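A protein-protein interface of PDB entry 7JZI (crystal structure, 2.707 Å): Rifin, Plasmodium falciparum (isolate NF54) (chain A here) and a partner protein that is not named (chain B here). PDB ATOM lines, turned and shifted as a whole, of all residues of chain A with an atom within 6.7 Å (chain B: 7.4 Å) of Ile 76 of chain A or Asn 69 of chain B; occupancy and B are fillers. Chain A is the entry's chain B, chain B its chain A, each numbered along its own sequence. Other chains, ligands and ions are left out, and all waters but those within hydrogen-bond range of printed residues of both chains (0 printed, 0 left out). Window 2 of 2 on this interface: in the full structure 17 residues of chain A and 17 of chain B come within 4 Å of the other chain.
Of the 8 printed residues of chain A, 4 touch a printed residue of chain B. Along chain A the printed residues that touch a printed residue of chain B span positions 73 to 76. Of the 15 printed residues of chain B, 4 touch a printed residue of chain A. Printed residues of chain B that touch a printed residue of chain A: Arg 39, Ile 65, Asn 69 and Asn 72. Along chain B the printed residues that touch a printed residue of chain A span positions 39 to 72. Among the printed residues, 5 pairs touch across the chains.
N of Asn 69 of chain B sits at hydrogen-bond distance from OD1 of Asn 72 of chain B. The side-chain hydroxyl (OG) of Ser 72 of chain A sits at hydrogen-bond distance from the backbone NH (N) of Thr 74 of chain A (3.0 Å). The guanidinium group of Arg 39 of chain B is in hydrogen-bond range of the backbone carbonyl oxygen of Asn 72 of chain B (3.2 Å). NH2 of Arg 39 of chain B is in hydrogen-bond range of O of Gly 71 of chain B (2.9 Å). The side-chain hydroxyl (OG) of Ser 72 of chain A lies within hydrogen-bond range of the backbone NH (N) of Tyr 75 of chain A (3.1 Å). OD1 of Asn 69 of chain B lies within hydrogen-bond range of N of Gly 71 of chain B.
Val 70 of chain A touches none of the printed residues of chain B. Of the printed residues of chain B, Thr 74 of chain A touches Ile 65 and Asn 72. Printed residues of chain B within 4 Å of Tyr 75 of chain A: Arg 39. Printed residues of chain A within 4 Å of Ile 65 of chain B: Thr 74. Of the printed residues of chain A, Asn 69 of chain B touches Ile 76.
CD of Arg 39 of chain B touches O of Ala 73 of chain A, at 3.9 Å. Ile 65 of chain B touches Thr 74 of chain A (CG2 to CG2, 3.3 Å). Tyr 75 of chain A touches Arg 39 of chain B. OD1 of Asn 69 of chain B touches CG2 of Ile 76 of chain A, 3.2 Å away.
ND2 of Asn 72 of chain B is in hydrogen-bond range of O of Thr 74 of chain A (3.3 Å).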
ATOM      1  N   VAL A  70      14.405  -9.588 -34.214  1.00  0.00           N
ATOM      2  CA  VAL A  70      14.173  -9.970 -32.825  1.00  0.00           C
ATOM      3  C   VAL A  70      13.119 -11.056 -32.690  1.00  0.00           C
ATOM      4  O   VAL A  70      12.958 -11.620 -31.600  1.00  0.00           O
ATOM      5  CB  VAL A  70      13.776  -8.777 -31.934  1.00  0.00           C
ATOM      6  CG1 VAL A  70      15.003  -7.945 -31.555  1.00  0.00           C
ATOM      7  CG2 VAL A  70      12.698  -7.942 -32.584  1.00  0.00           C
ATOM      8  N   SER A  72      12.985 -13.659 -35.028  1.00  0.00           N
ATOM      9  CA  SER A  72      13.409 -14.756 -35.876  1.00  0.00           C
ATOM     10  C   SER A  72      13.421 -16.063 -35.089  1.00  0.00           C
ATOM     11  O   SER A  72      13.442 -16.080 -33.856  1.00  0.00           O
ATOM     12  CB  SER A  72      14.796 -14.474 -36.454  1.00  0.00           C
ATOM     13  OG  SER A  72      15.801 -15.006 -35.614  1.00  0.00           O
ATOM     14  N   ALA A  73      13.420 -17.173 -35.827  1.00  0.00           N
ATOM     15  CA  ALA A  73      13.519 -18.487 -35.198  1.00  0.00           C
ATOM     16  C   ALA A  73      14.892 -18.703 -34.594  1.00  0.00           C
ATOM     17  O   ALA A  73      15.081 -19.615 -33.785  1.00  0.00           O
ATOM     18  CB  ALA A  73      13.230 -19.590 -36.207  1.00  0.00           C
ATOM     19  N   THR A  74      15.854 -17.897 -35.014  1.00  0.00           N
ATOM     20  CA  THR A  74      17.243 -17.910 -34.577  1.00  0.00           C
ATOM     21  C   THR A  74      17.472 -17.226 -33.226  1.00  0.00           C
ATOM     22  O   THR A  74      18.382 -17.622 -32.480  1.00  0.00           O
ATOM     23  CB  THR A  74      18.085 -17.208 -35.659  1.00  0.00           C
ATOM     24  OG1 THR A  74      17.666 -17.646 -36.959  1.00  0.00           O
ATOM     25  CG2 THR A  74      19.546 -17.484 -35.506  1.00  0.00           C
ATOM     26  N   TYR A  75      16.622 -16.266 -32.882  1.00  0.00           N
ATOM     27  CA  TYR A  75      16.891 -15.329 -31.802  1.00  0.00           C
ATOM     28  C   TYR A  75      17.020 -16.025 -30.448  1.00  0.00           C
ATOM     29  O   TYR A  75      16.372 -17.039 -30.178  1.00  0.00           O
ATOM     30  CB  TYR A  75      15.790 -14.278 -31.764  1.00  0.00           C
ATOM     31  CG  TYR A  75      16.059 -13.113 -30.850  1.00  0.00           C
ATOM     32  CD1 TYR A  75      16.749 -12.006 -31.315  1.00  0.00           C
ATOM     33  CD2 TYR A  75      15.592 -13.097 -29.547  1.00  0.00           C
ATOM     34  CE1 TYR A  75      17.002 -10.927 -30.500  1.00  0.00           C
ATOM     35  CE2 TYR A  75      15.835 -12.020 -28.720  1.00  0.00           C
ATOM     36  CZ  TYR A  75      16.540 -10.936 -29.203  1.00  0.00           C
ATOM     37  OH  TYR A  75      16.787  -9.860 -28.380  1.00  0.00           O
ATOM     38  N   ILE A  76      17.888 -15.470 -29.604  1.00  0.00           N
ATOM     39  CA  ILE A  76      18.160 -16.008 -28.274  1.00  0.00           C
ATOM     40  C   ILE A  76      17.267 -15.270 -27.289  1.00  0.00           C
ATOM     41  O   ILE A  76      17.492 -14.094 -26.996  1.00  0.00           O
ATOM     42  CB  ILE A  76      19.637 -15.843 -27.889  1.00  0.00           C
ATOM     43  CG1 ILE A  76      20.556 -16.243 -29.047  1.00  0.00           C
ATOM     44  CG2 ILE A  76      19.945 -16.605 -26.610  1.00  0.00           C
ATOM     45  CD1 ILE A  76      21.096 -15.056 -29.839  1.00  0.00           C
ATOM     46  N   GLY A  77      16.251 -15.955 -26.782  1.00  0.00           N
ATOM     47  CA  GLY A  77      15.335 -15.374 -25.826  1.00  0.00           C
ATOM     48  C   GLY A  77      14.046 -14.906 -26.476  1.00  0.00           C
ATOM     49  O   GLY A  77      13.924 -14.797 -27.698  1.00  0.00           O
ATOM     50  N   ILE A  78      13.058 -14.626 -25.627  1.00  0.00           N
ATOM     51  CA  ILE A  78      11.740 -14.191 -26.075  1.00  0.00           C
ATOM     52  C   ILE A  78      11.639 -12.686 -25.872  1.00  0.00           C
ATOM     53  O   ILE A  78      12.122 -12.148 -24.870  1.00  0.00           O
ATOM     54  CB  ILE A  78      10.621 -14.948 -25.335  1.00  0.00           C
ATOM     55  CG1 ILE A  78      10.567 -16.403 -25.810  1.00  0.00           C
ATOM     56  CG2 ILE A  78       9.275 -14.306 -25.592  1.00  0.00           C
ATOM     57  CD1 ILE A  78      10.987 -17.414 -24.761  1.00  0.00           C
ATOM     58  N   PRO B  17      25.393 -30.398 -28.366  1.00  0.00           N
ATOM     59  CA  PRO B  17      25.994 -29.811 -27.164  1.00  0.00           C
ATOM     60  C   PRO B  17      25.997 -28.294 -27.254  1.00  0.00           C
ATOM     61  O   PRO B  17      26.074 -27.720 -28.343  1.00  0.00           O
ATOM     62  CB  PRO B  17      27.425 -30.366 -27.171  1.00  0.00           C
ATOM     63  CG  PRO B  17      27.407 -31.515 -28.134  1.00  0.00           C
ATOM     64  CD  PRO B  17      26.373 -31.165 -29.154  1.00  0.00           C
ATOM     65  N   LEU B  18      25.900 -27.647 -26.089  1.00  0.00           N
ATOM     66  CA  LEU B  18      25.949 -26.193 -26.052  1.00  0.00           C
ATOM     67  C   LEU B  18      27.195 -25.720 -26.785  1.00  0.00           C
ATOM     68  O   LEU B  18      28.263 -26.327 -26.687  1.00  0.00           O
ATOM     69  CB  LEU B  18      25.942 -25.705 -24.604  1.00  0.00           C
ATOM     70  CG  LEU B  18      25.259 -24.379 -24.244  1.00  0.00           C
ATOM     71  CD1 LEU B  18      24.974 -24.303 -22.742  1.00  0.00           C
ATOM     72  CD2 LEU B  18      26.088 -23.166 -24.689  1.00  0.00           C
ATOM     73  N   GLY B  19      27.066 -24.633 -27.533  1.00  0.00           N
ATOM     74  CA  GLY B  19      28.213 -24.081 -28.221  1.00  0.00           C
ATOM     75  C   GLY B  19      28.504 -24.655 -29.598  1.00  0.00           C
ATOM     76  O   GLY B  19      29.321 -24.080 -30.341  1.00  0.00           O
ATOM     77  N   SER B  20      27.921 -25.797 -29.947  1.00  0.00           N
ATOM     78  CA  SER B  20      28.105 -26.319 -31.291  1.00  0.00           C
ATOM     79  C   SER B  20      27.053 -25.751 -32.252  1.00  0.00           C
ATOM     80  O   SER B  20      26.020 -25.220 -31.842  1.00  0.00           O
ATOM     81  CB  SER B  20      28.056 -27.841 -31.273  1.00  0.00           C
ATOM     82  OG  SER B  20      28.151 -28.347 -32.586  1.00  0.00           O
ATOM     83  N   ARG B  39       9.001 -21.917 -34.660  1.00  0.00           N
ATOM     84  CA  ARG B  39       9.131 -22.552 -33.361  1.00  0.00           C
ATOM     85  C   ARG B  39       7.739 -22.879 -32.829  1.00  0.00           C
ATOM     86  O   ARG B  39       6.733 -22.746 -33.533  1.00  0.00           O
ATOM     87  CB  ARG B  39       9.879 -21.663 -32.367  1.00  0.00           C
ATOM     88  CG  ARG B  39      11.041 -20.895 -32.931  1.00  0.00           C
ATOM     89  CD  ARG B  39      11.812 -20.200 -31.823  1.00  0.00           C
ATOM     90  NE  ARG B  39      12.374 -21.157 -30.869  1.00  0.00           N
ATOM     91  CZ  ARG B  39      13.261 -20.848 -29.926  1.00  0.00           C
ATOM     92  NH1 ARG B  39      13.701 -19.602 -29.812  1.00  0.00           N
ATOM     93  NH2 ARG B  39      13.706 -21.783 -29.094  1.00  0.00           N
ATOM     94  N   ILE B  65      22.321 -22.263 -37.151  1.00  0.00           N
ATOM     95  CA  ILE B  65      22.847 -21.460 -36.053  1.00  0.00           C
ATOM     96  C   ILE B  65      24.265 -21.941 -35.764  1.00  0.00           C
ATOM     97  O   ILE B  65      24.512 -23.152 -35.628  1.00  0.00           O
ATOM     98  CB  ILE B  65      21.931 -21.468 -34.810  1.00  0.00           C
ATOM     99  CG1 ILE B  65      21.277 -22.819 -34.508  1.00  0.00           C
ATOM    100  CG2 ILE B  65      20.837 -20.477 -34.957  1.00  0.00           C
ATOM    101  CD1 ILE B  65      22.195 -23.805 -33.973  1.00  0.00           C
ATOM    102  N   SER B  67      26.271 -21.532 -33.161  1.00  0.00           N
ATOM    103  CA  SER B  67      26.403 -22.201 -31.875  1.00  0.00           C
ATOM    104  C   SER B  67      25.131 -22.030 -31.053  1.00  0.00           C
ATOM    105  O   SER B  67      24.629 -20.912 -30.864  1.00  0.00           O
ATOM    106  CB  SER B  67      27.611 -21.663 -31.114  1.00  0.00           C
ATOM    107  OG  SER B  67      27.175 -20.662 -30.231  1.00  0.00           O
ATOM    108  N   VAL B  68      24.690 -23.157 -30.488  1.00  0.00           N
ATOM    109  CA  VAL B  68      23.465 -23.217 -29.709  1.00  0.00           C
ATOM    110  C   VAL B  68      23.705 -22.661 -28.308  1.00  0.00           C
ATOM    111  O   VAL B  68      24.830 -22.627 -27.804  1.00  0.00           O
ATOM    112  CB  VAL B  68      22.902 -24.645 -29.644  1.00  0.00           C
ATOM    113  CG1 VAL B  68      22.919 -25.272 -31.011  1.00  0.00           C
ATOM    114  CG2 VAL B  68      23.719 -25.483 -28.677  1.00  0.00           C
ATOM    115  N   ASN B  69      22.618 -22.205 -27.683  1.00  0.00           N
ATOM    116  CA  ASN B  69      22.511 -22.061 -26.236  1.00  0.00           C
ATOM    117  C   ASN B  69      21.094 -22.469 -25.849  1.00  0.00           C
ATOM    118  O   ASN B  69      20.227 -22.669 -26.707  1.00  0.00           O
ATOM    119  CB  ASN B  69      22.877 -20.646 -25.753  1.00  0.00           C
ATOM    120  CG  ASN B  69      21.905 -19.588 -26.226  1.00  0.00           C
ATOM    121  OD1 ASN B  69      20.711 -19.623 -25.914  1.00  0.00           O
ATOM    122  ND2 ASN B  69      22.420 -18.626 -26.981  1.00  0.00           N
ATOM    123  N   ALA B  70      20.874 -22.602 -24.538  1.00  0.00           N
ATOM    124  CA  ALA B  70      19.646 -23.185 -24.006  1.00  0.00           C
ATOM    125  C   ALA B  70      18.387 -22.450 -24.450  1.00  0.00           C
ATOM    126  O   ALA B  70      17.288 -22.989 -24.285  1.00  0.00           O
ATOM    127  CB  ALA B  70      19.711 -23.222 -22.477  1.00  0.00           C
ATOM    128  N   GLY B  71      18.509 -21.228 -24.973  1.00  0.00           N
ATOM    129  CA  GLY B  71      17.349 -20.552 -25.528  1.00  0.00           C
ATOM    130  C   GLY B  71      16.948 -21.037 -26.907  1.00  0.00           C
ATOM    131  O   GLY B  71      15.829 -20.756 -27.349  1.00  0.00           O
ATOM    132  N   ASN B  72      17.838 -21.751 -27.599  1.00  0.00           N
ATOM    133  CA  ASN B  72      17.525 -22.289 -28.918  1.00  0.00           C
ATOM    134  C   ASN B  72      16.698 -23.567 -28.863  1.00  0.00           C
ATOM    135  O   ASN B  72      16.014 -23.888 -29.844  1.00  0.00           O
ATOM    136  CB  ASN B  72      18.812 -22.547 -29.705  1.00  0.00           C
ATOM    137  CG  ASN B  72      19.414 -21.278 -30.258  1.00  0.00           C
ATOM    138  OD1 ASN B  72      20.597 -21.001 -30.066  1.00  0.00           O
ATOM    139  ND2 ASN B  72      18.597 -20.493 -30.951  1.00  0.00           N
ATOM    140  N   ALA B  73      16.756 -24.309 -27.761  1.00  0.00           N
ATOM    141  CA  ALA B  73      16.073 -25.592 -27.684  1.00  0.00           C
ATOM    142  C   ALA B  73      14.563 -25.416 -27.757  1.00  0.00           C
ATOM    143  O   ALA B  73      13.999 -24.448 -27.236  1.00  0.00           O
ATOM    144  CB  ALA B  73      16.439 -26.320 -26.390  1.00  0.00           C
ATOM    145  N   LEU B  95      14.625 -29.975 -30.938  1.00  0.00           N
ATOM    146  CA  LEU B  95      16.067 -30.032 -30.730  1.00  0.00           C
ATOM    147  C   LEU B  95      16.367 -29.621 -29.297  1.00  0.00           C
ATOM    148  O   LEU B  95      15.868 -28.596 -28.810  1.00  0.00           O
ATOM    149  CB  LEU B  95      16.919 -29.235 -31.722  1.00  0.00           C
ATOM    150  CG  LEU B  95      18.416 -29.088 -31.446  1.00  0.00           C
ATOM    151  CD1 LEU B  95      19.038 -29.162 -32.867  1.00  0.00           C
ATOM    152  CD2 LEU B  95      18.837 -27.835 -30.688  1.00  0.00           C
ATOM    153  N   VAL B  97      19.454 -29.162 -26.243  1.00  0.00           N
ATOM    154  CA  VAL B  97      20.843 -28.757 -26.055  1.00  0.00           C
ATOM    155  C   VAL B  97      21.416 -29.480 -24.842  1.00  0.00           C
ATOM    156  O   VAL B  97      20.706 -29.746 -23.862  1.00  0.00           O
ATOM    157  CB  VAL B  97      20.971 -27.227 -25.908  1.00  0.00           C
ATOM    158  CG1 VAL B  97      20.256 -26.523 -27.050  1.00  0.00           C
ATOM    159  CG2 VAL B  97      20.421 -26.762 -24.562  1.00  0.00           C
